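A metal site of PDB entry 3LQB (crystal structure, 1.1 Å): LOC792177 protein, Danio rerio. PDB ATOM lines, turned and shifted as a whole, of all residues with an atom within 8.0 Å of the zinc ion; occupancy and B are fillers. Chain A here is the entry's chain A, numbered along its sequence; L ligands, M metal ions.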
ATOM      1  N   CYS A  71     -27.318  28.981  12.165  1.00  0.00           N
ATOM      2  CA  CYS A  71     -26.752  27.707  12.576  1.00  0.00           C
ATOM      3  C   CYS A  71     -26.182  27.092  11.302  1.00  0.00           C
ATOM      4  O   CYS A  71     -26.912  26.887  10.341  1.00  0.00           O
ATOM      5  CB  CYS A  71     -27.817  26.772  13.153  1.00  0.00           C
ATOM      6  SG  CYS A  71     -29.261  27.511  13.962  1.00  0.00           S
ATOM      7  N   TYR A  72     -24.881  26.872  11.253  1.00  0.00           N
ATOM      8  CA  TYR A  72     -24.255  26.348  10.045  1.00  0.00           C
ATOM      9  C   TYR A  72     -22.883  25.733  10.317  1.00  0.00           C
ATOM     10  O   TYR A  72     -22.279  25.958  11.371  1.00  0.00           O
ATOM     11  CB  TYR A  72     -24.149  27.416   8.929  1.00  0.00           C
ATOM     12  CG  TYR A  72     -23.311  28.638   9.200  1.00  0.00           C
ATOM     13  CD1 TYR A  72     -21.924  28.603   9.124  1.00  0.00           C
ATOM     14  CD2 TYR A  72     -23.925  29.874   9.457  1.00  0.00           C
ATOM     15  CE1 TYR A  72     -21.170  29.737   9.331  1.00  0.00           C
ATOM     16  CE2 TYR A  72     -23.183  31.001   9.693  1.00  0.00           C
ATOM     17  CZ  TYR A  72     -21.813  30.935   9.624  1.00  0.00           C
ATOM     18  OH  TYR A  72     -21.050  32.079   9.827  1.00  0.00           O
ATOM     19  N   SER A  73     -22.416  24.951   9.355  1.00  0.00           N
ATOM     20  CA  SER A  73     -21.090  24.367   9.374  1.00  0.00           C
ATOM     21  C   SER A  73     -20.660  24.098   7.953  1.00  0.00           C
ATOM     22  O   SER A  73     -21.490  23.907   7.054  1.00  0.00           O
ATOM     23  CB  SER A  73     -21.135  23.024  10.132  1.00  0.00           C
ATOM     24  OG  SER A  73     -19.908  22.339  10.100  1.00  0.00           O
ATOM     25  N   ILE A  75     -19.015  21.383   5.306  1.00  0.00           N
ATOM     26  CA  ILE A  75     -19.171  19.927   5.092  1.00  0.00           C
ATOM     27  C   ILE A  75     -17.797  19.266   4.992  1.00  0.00           C
ATOM     28  O   ILE A  75     -17.017  19.533   4.072  1.00  0.00           O
ATOM     29  CB  ILE A  75     -20.020  19.604   3.842  1.00  0.00           C
ATOM     30  CG1 ILE A  75     -21.330  20.399   3.887  1.00  0.00           C
ATOM     31  CG2 ILE A  75     -20.306  18.086   3.758  1.00  0.00           C
ATOM     32  CD1 ILE A  75     -22.441  19.866   3.057  1.00  0.00           C
ATOM     33  N   ILE A  96     -29.574  20.609  17.316  1.00  0.00           N
ATOM     34  CA  ILE A  96     -29.045  21.520  16.309  1.00  0.00           C
ATOM     35  C   ILE A  96     -27.514  21.468  16.278  1.00  0.00           C
ATOM     36  O   ILE A  96     -26.909  21.394  15.223  1.00  0.00           O
ATOM     37  CB  ILE A  96     -29.575  22.949  16.430  1.00  0.00           C
ATOM     38  CG1 ILE A  96     -31.092  22.941  16.098  1.00  0.00           C
ATOM     39  CG2 ILE A  96     -28.807  23.901  15.523  1.00  0.00           C
ATOM     40  CD1 ILE A  96     -31.751  24.283  16.131  1.00  0.00           C
ATOM     41  N   HIS A  99     -26.458  18.378  14.568  1.00  0.00           N
ATOM     42  CA  HIS A  99     -26.669  18.518  13.158  1.00  0.00           C
ATOM     43  C   HIS A  99     -25.491  19.249  12.525  1.00  0.00           C
ATOM     44  O   HIS A  99     -24.921  18.790  11.521  1.00  0.00           O
ATOM     45  CB  HIS A  99     -27.974  19.291  12.932  1.00  0.00           C
ATOM     46  CG  HIS A  99     -28.288  19.655  11.508  1.00  0.00           C
ATOM     47  ND1 HIS A  99     -29.300  19.069  10.797  1.00  0.00           N
ATOM     48  CD2 HIS A  99     -27.730  20.567  10.675  1.00  0.00           C
ATOM     49  CE1 HIS A  99     -29.367  19.619   9.586  1.00  0.00           C
ATOM     50  NE2 HIS A  99     -28.428  20.547   9.477  1.00  0.00           N
ATOM     51  N   GLU A 100     -25.055  20.368  13.107  1.00  0.00           N
ATOM     52  CA  GLU A 100     -23.928  21.107  12.539  1.00  0.00           C
ATOM     53  C   GLU A 100     -22.618  20.320  12.658  1.00  0.00           C
ATOM     54  O   GLU A 100     -21.836  20.301  11.718  1.00  0.00           O
ATOM     55  CB  GLU A 100     -23.777  22.483  13.209  1.00  0.00           C
ATOM     56  CG  GLU A 100     -25.024  23.357  13.242  1.00  0.00           C
ATOM     57  CD  GLU A 100     -25.761  23.497  11.929  1.00  0.00           C
ATOM     58  OE1 GLU A 100     -25.201  23.258  10.846  1.00  0.00           O
ATOM     59  OE2 GLU A 100     -26.962  23.850  12.022  1.00  0.00           O
ATOM     60  N   ASN A 102     -22.328  17.153  12.632  1.00  0.00           N
ATOM     61  CA  ASN A 102     -22.408  16.070  11.656  1.00  0.00           C
ATOM     62  C   ASN A 102     -22.091  16.562  10.238  1.00  0.00           C
ATOM     63  O   ASN A 102     -21.461  15.852   9.448  1.00  0.00           O
ATOM     64  CB  ASN A 102     -23.758  15.375  11.721  1.00  0.00           C
ATOM     65  CG  ASN A 102     -23.684  13.931  11.255  1.00  0.00           C
ATOM     66  OD1 ASN A 102     -22.679  13.235  11.468  1.00  0.00           O
ATOM     67  ND2 ASN A 102     -24.718  13.515  10.540  1.00  0.00           N
ATOM     68  N   HIS A 103     -22.468  17.794   9.907  1.00  0.00           N
ATOM     69  CA  HIS A 103     -21.986  18.386   8.668  1.00  0.00           C
ATOM     70  C   HIS A 103     -20.462  18.393   8.654  1.00  0.00           C
ATOM     71  O   HIS A 103     -19.844  17.985   7.676  1.00  0.00           O
ATOM     72  CB  HIS A 103     -22.461  19.828   8.489  1.00  0.00           C
ATOM     73  CG  HIS A 103     -23.886  19.997   8.039  1.00  0.00           C
ATOM     74  ND1 HIS A 103     -24.416  19.350   6.938  1.00  0.00           N
ATOM     75  CD2 HIS A 103     -24.854  20.854   8.455  1.00  0.00           C
ATOM     76  CE1 HIS A 103     -25.656  19.786   6.741  1.00  0.00           C
ATOM     77  NE2 HIS A 103     -25.939  20.714   7.622  1.00  0.00           N
ATOM     78  N   PHE A 107     -21.248  15.112   6.221  1.00  0.00           N
ATOM     79  CA  PHE A 107     -22.602  14.743   5.810  1.00  0.00           C
ATOM     80  C   PHE A 107     -23.418  15.922   5.308  1.00  0.00           C
ATOM     81  O   PHE A 107     -23.385  16.998   5.902  1.00  0.00           O
ATOM     82  CB  PHE A 107     -23.337  14.033   6.966  1.00  0.00           C
ATOM     83  CG  PHE A 107     -22.688  12.733   7.284  1.00  0.00           C
ATOM     84  CD1 PHE A 107     -22.946  11.612   6.522  1.00  0.00           C
ATOM     85  CD2 PHE A 107     -21.754  12.613   8.291  1.00  0.00           C
ATOM     86  CE1 PHE A 107     -22.284  10.416   6.720  1.00  0.00           C
ATOM     87  CE2 PHE A 107     -21.104  11.420   8.520  1.00  0.00           C
ATOM     88  CZ  PHE A 107     -21.370  10.309   7.724  1.00  0.00           C
ATOM     89  N   TYR A 108     -24.154  15.687   4.229  1.00  0.00           N
ATOM     90  CA  TYR A 108     -25.118  16.619   3.660  1.00  0.00           C
ATOM     91  C   TYR A 108     -26.495  16.415   4.272  1.00  0.00           C
ATOM     92  O   TYR A 108     -26.774  15.451   4.993  1.00  0.00           O
ATOM     93  CB  TYR A 108     -25.259  16.416   2.144  1.00  0.00           C
ATOM     94  CG  TYR A 108     -24.095  16.642   1.263  1.00  0.00           C
ATOM     95  CD1 TYR A 108     -23.639  17.920   0.970  1.00  0.00           C
ATOM     96  CD2 TYR A 108     -23.484  15.561   0.623  1.00  0.00           C
ATOM     97  CE1 TYR A 108     -22.592  18.121   0.075  1.00  0.00           C
ATOM     98  CE2 TYR A 108     -22.482  15.750  -0.288  1.00  0.00           C
ATOM     99  CZ  TYR A 108     -22.011  17.020  -0.554  1.00  0.00           C
ATOM    100  OH  TYR A 108     -20.999  17.225  -1.453  1.00  0.00           O
ATOM    101  N   HIS A 109     -27.398  17.315   3.955  1.00  0.00           N
ATOM    102  CA  HIS A 109     -28.803  17.137   4.290  1.00  0.00           C
ATOM    103  C   HIS A 109     -29.377  15.891   3.615  1.00  0.00           C
ATOM    104  O   HIS A 109     -29.002  15.500   2.516  1.00  0.00           O
ATOM    105  CB  HIS A 109     -29.589  18.360   3.848  1.00  0.00           C
ATOM    106  CG  HIS A 109     -29.223  19.572   4.615  1.00  0.00           C
ATOM    107  ND1 HIS A 109     -28.912  20.778   4.031  1.00  0.00           N
ATOM    108  CD2 HIS A 109     -29.057  19.740   5.944  1.00  0.00           C
ATOM    109  CE1 HIS A 109     -28.561  21.641   4.982  1.00  0.00           C
ATOM    110  NE2 HIS A 109     -28.631  21.032   6.155  1.00  0.00           N
ATOM    111  N   GLU A 110     -30.342  15.281   4.297  1.00  0.00           N
ATOM    112  CA  GLU A 110     -30.941  14.044   3.831  1.00  0.00           C
ATOM    113  C   GLU A 110     -31.614  14.220   2.472  1.00  0.00           C
ATOM    114  O   GLU A 110     -31.468  13.386   1.567  1.00  0.00           O
ATOM    115  CB  GLU A 110     -31.908  13.487   4.859  1.00  0.00           C
ATOM    116  CG  GLU A 110     -32.375  12.043   4.571  1.00  0.00           C
ATOM    117  CD  GLU A 110     -31.277  11.016   4.702  1.00  0.00           C
ATOM    118  OE1 GLU A 110     -30.153  11.383   5.097  1.00  0.00           O
ATOM    119  OE2 GLU A 110     -31.537   9.826   4.428  1.00  0.00           O
ATOM    120  N   GLN A 111     -32.389  15.290   2.326  1.00  0.00           N
ATOM    121  CA  GLN A 111     -33.124  15.474   1.076  1.00  0.00           C
ATOM    122  C   GLN A 111     -32.228  15.919  -0.088  1.00  0.00           C
ATOM    123  O   GLN A 111     -32.704  16.082  -1.205  1.00  0.00           O
ATOM    124  CB  GLN A 111     -34.297  16.416   1.256  1.00  0.00           C
ATOM    125  CG  GLN A 111     -33.962  17.902   1.365  1.00  0.00           C
ATOM    126  CD  GLN A 111     -33.322  18.309   2.658  1.00  0.00           C
ATOM    127  OE1 GLN A 111     -33.545  17.697   3.708  1.00  0.00           O
ATOM    128  NE2 GLN A 111     -32.564  19.380   2.628  1.00  0.00           N
ATOM    129  N   ASN A 134     -30.820  25.640  -1.544  1.00  0.00           N
ATOM    130  CA  ASN A 134     -30.771  24.774  -0.389  1.00  0.00           C
ATOM    131  C   ASN A 134     -31.454  23.439  -0.649  1.00  0.00           C
ATOM    132  O   ASN A 134     -31.347  22.544   0.201  1.00  0.00           O
ATOM    133  CB  ASN A 134     -31.487  25.444   0.776  1.00  0.00           C
ATOM    134  CG  ASN A 134     -30.768  26.668   1.320  1.00  0.00           C
ATOM    135  OD1 ASN A 134     -29.721  26.562   1.956  1.00  0.00           O
ATOM    136  ND2 ASN A 134     -31.337  27.838   1.064  1.00  0.00           N
ATOM    137  N   LEU A 152     -31.535  13.343  11.385  1.00  0.00           N
ATOM    138  CA  LEU A 152     -31.298  14.666  11.947  1.00  0.00           C
ATOM    139  C   LEU A 152     -30.924  15.655  10.867  1.00  0.00           C
ATOM    140  O   LEU A 152     -31.004  16.871  11.058  1.00  0.00           O
ATOM    141  CB  LEU A 152     -30.176  14.552  12.973  1.00  0.00           C
ATOM    142  CG  LEU A 152     -29.869  15.806  13.762  1.00  0.00           C
ATOM    143  CD1 LEU A 152     -31.039  16.110  14.729  1.00  0.00           C
ATOM    144  CD2 LEU A 152     -28.579  15.670  14.530  1.00  0.00           C
ATOM    145  N   MET A 153     -30.509  15.132   9.700  1.00  0.00           N
ATOM    146  CA  MET A 153     -30.082  15.956   8.587  1.00  0.00           C
ATOM    147  C   MET A 153     -31.220  16.318   7.614  1.00  0.00           C
ATOM    148  O   MET A 153     -30.960  16.997   6.610  1.00  0.00           O
ATOM    149  CB  MET A 153     -28.943  15.255   7.836  1.00  0.00           C
ATOM    150  CG  MET A 153     -27.828  14.769   8.738  1.00  0.00           C
ATOM    151  SD  MET A 153     -27.166  16.004   9.883  1.00  0.00           S
ATOM    152  CE  MET A 153     -26.383  17.170   8.754  1.00  0.00           C
ATOM    153  N   HIS A 154     -32.446  15.877   7.888  1.00  0.00           N
ATOM    154  CA  HIS A 154     -33.584  16.164   6.998  1.00  0.00           C
ATOM    155  C   HIS A 154     -34.240  17.482   7.354  1.00  0.00           C
ATOM    156  O   HIS A 154     -34.529  17.732   8.519  1.00  0.00           O
ATOM    157  CB  HIS A 154     -34.634  15.050   7.070  1.00  0.00           C
ATOM    158  CG  HIS A 154     -35.455  14.878   5.830  1.00  0.00           C
ATOM    159  ND1 HIS A 154     -36.310  15.837   5.350  1.00  0.00           N
ATOM    160  CD2 HIS A 154     -35.515  13.850   4.950  1.00  0.00           C
ATOM    161  CE1 HIS A 154     -36.860  15.396   4.226  1.00  0.00           C
ATOM    162  NE2 HIS A 154     -36.379  14.200   3.951  1.00  0.00           N
ATOM    163  N   TYR A 155     -34.498  18.328   6.360  1.00  0.00           N
ATOM    164  CA  TYR A 155     -35.314  19.506   6.562  1.00  0.00           C
ATOM    165  C   TYR A 155     -36.749  19.144   6.973  1.00  0.00           C
ATOM    166  O   TYR A 155     -37.284  18.071   6.607  1.00  0.00           O
ATOM    167  CB  TYR A 155     -35.428  20.318   5.286  1.00  0.00           C
ATOM    168  CG  TYR A 155     -34.237  21.141   4.884  1.00  0.00           C
ATOM    169  CD1 TYR A 155     -33.081  21.258   5.656  1.00  0.00           C
ATOM    170  CD2 TYR A 155     -34.307  21.872   3.700  1.00  0.00           C
ATOM    171  CE1 TYR A 155     -32.012  22.031   5.218  1.00  0.00           C
ATOM    172  CE2 TYR A 155     -33.264  22.653   3.280  1.00  0.00           C
ATOM    173  CZ  TYR A 155     -32.118  22.740   4.052  1.00  0.00           C
ATOM    174  OH  TYR A 155     -31.076  23.528   3.605  1.00  0.00           O
ATOM    175  N   ARG A 182     -35.282  17.479  15.397  1.00  0.00           N
ATOM    176  CA  ARG A 182     -33.996  17.969  15.889  1.00  0.00           C
ATOM    177  C   ARG A 182     -33.768  17.520  17.317  1.00  0.00           C
ATOM    178  O   ARG A 182     -33.144  18.230  18.107  1.00  0.00           O
ATOM    179  CB  ARG A 182     -33.825  19.487  15.708  1.00  0.00           C
ATOM    180  CG  ARG A 182     -33.759  19.928  14.232  1.00  0.00           C
ATOM    181  CD  ARG A 182     -32.490  19.463  13.516  1.00  0.00           C
ATOM    182  NE  ARG A 182     -32.407  19.927  12.140  1.00  0.00           N
ATOM    183  CZ  ARG A 182     -32.965  19.321  11.089  1.00  0.00           C
ATOM    184  NH1 ARG A 182     -33.697  18.223  11.286  1.00  0.00           N
ATOM    185  NH2 ARG A 182     -32.818  19.803   9.853  1.00  0.00           N
HETATM  186  S1  LIG L   1     -28.628  24.178   8.824  1.00  0.00           S
HETATM  187  O1  LIG L   1     -28.891  24.103  10.296  1.00  0.00           O
HETATM  188  O2  LIG L   1     -28.382  25.572   8.377  1.00  0.00           O
HETATM  189  O3  LIG L   1     -27.399  23.433   8.431  1.00  0.00           O
HETATM  190  O4  LIG L   1     -29.688  23.425   8.137  1.00  0.00           O
HETATM  191 ZN    ZN M   1     -27.769  21.622   7.882  1.00  0.00          ZN
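A ring nitrogen (ND1) of His 99 lies within hydrogen-bond range of the guanidinium group (NE) of Arg 182. O of Leu 152 is in hydrogen-bond range of ND1 of His 99, at 2.8 Å. A ring nitrogen (ND1) of His 103 lies within hydrogen-bond range of the backbone carbonyl oxygen (O) of Phe 107 (2.8 Å).
The nearest printed residue that does not touch the zinc ion is Glu 100 (4.2 Å).
The zinc ion is bound by an oxygen (O3) of the ligand (1.9 Å), a ring nitrogen (NE2) of His 109 (2.0 Å), a ring nitrogen (NE2) of His 99 (2.0 Å) and a ring nitrogen (NE2) of His 103 (2.1 Å). Slightly farther from the zinc ion lies an oxygen (O4) of the ligand (2.6 Å).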
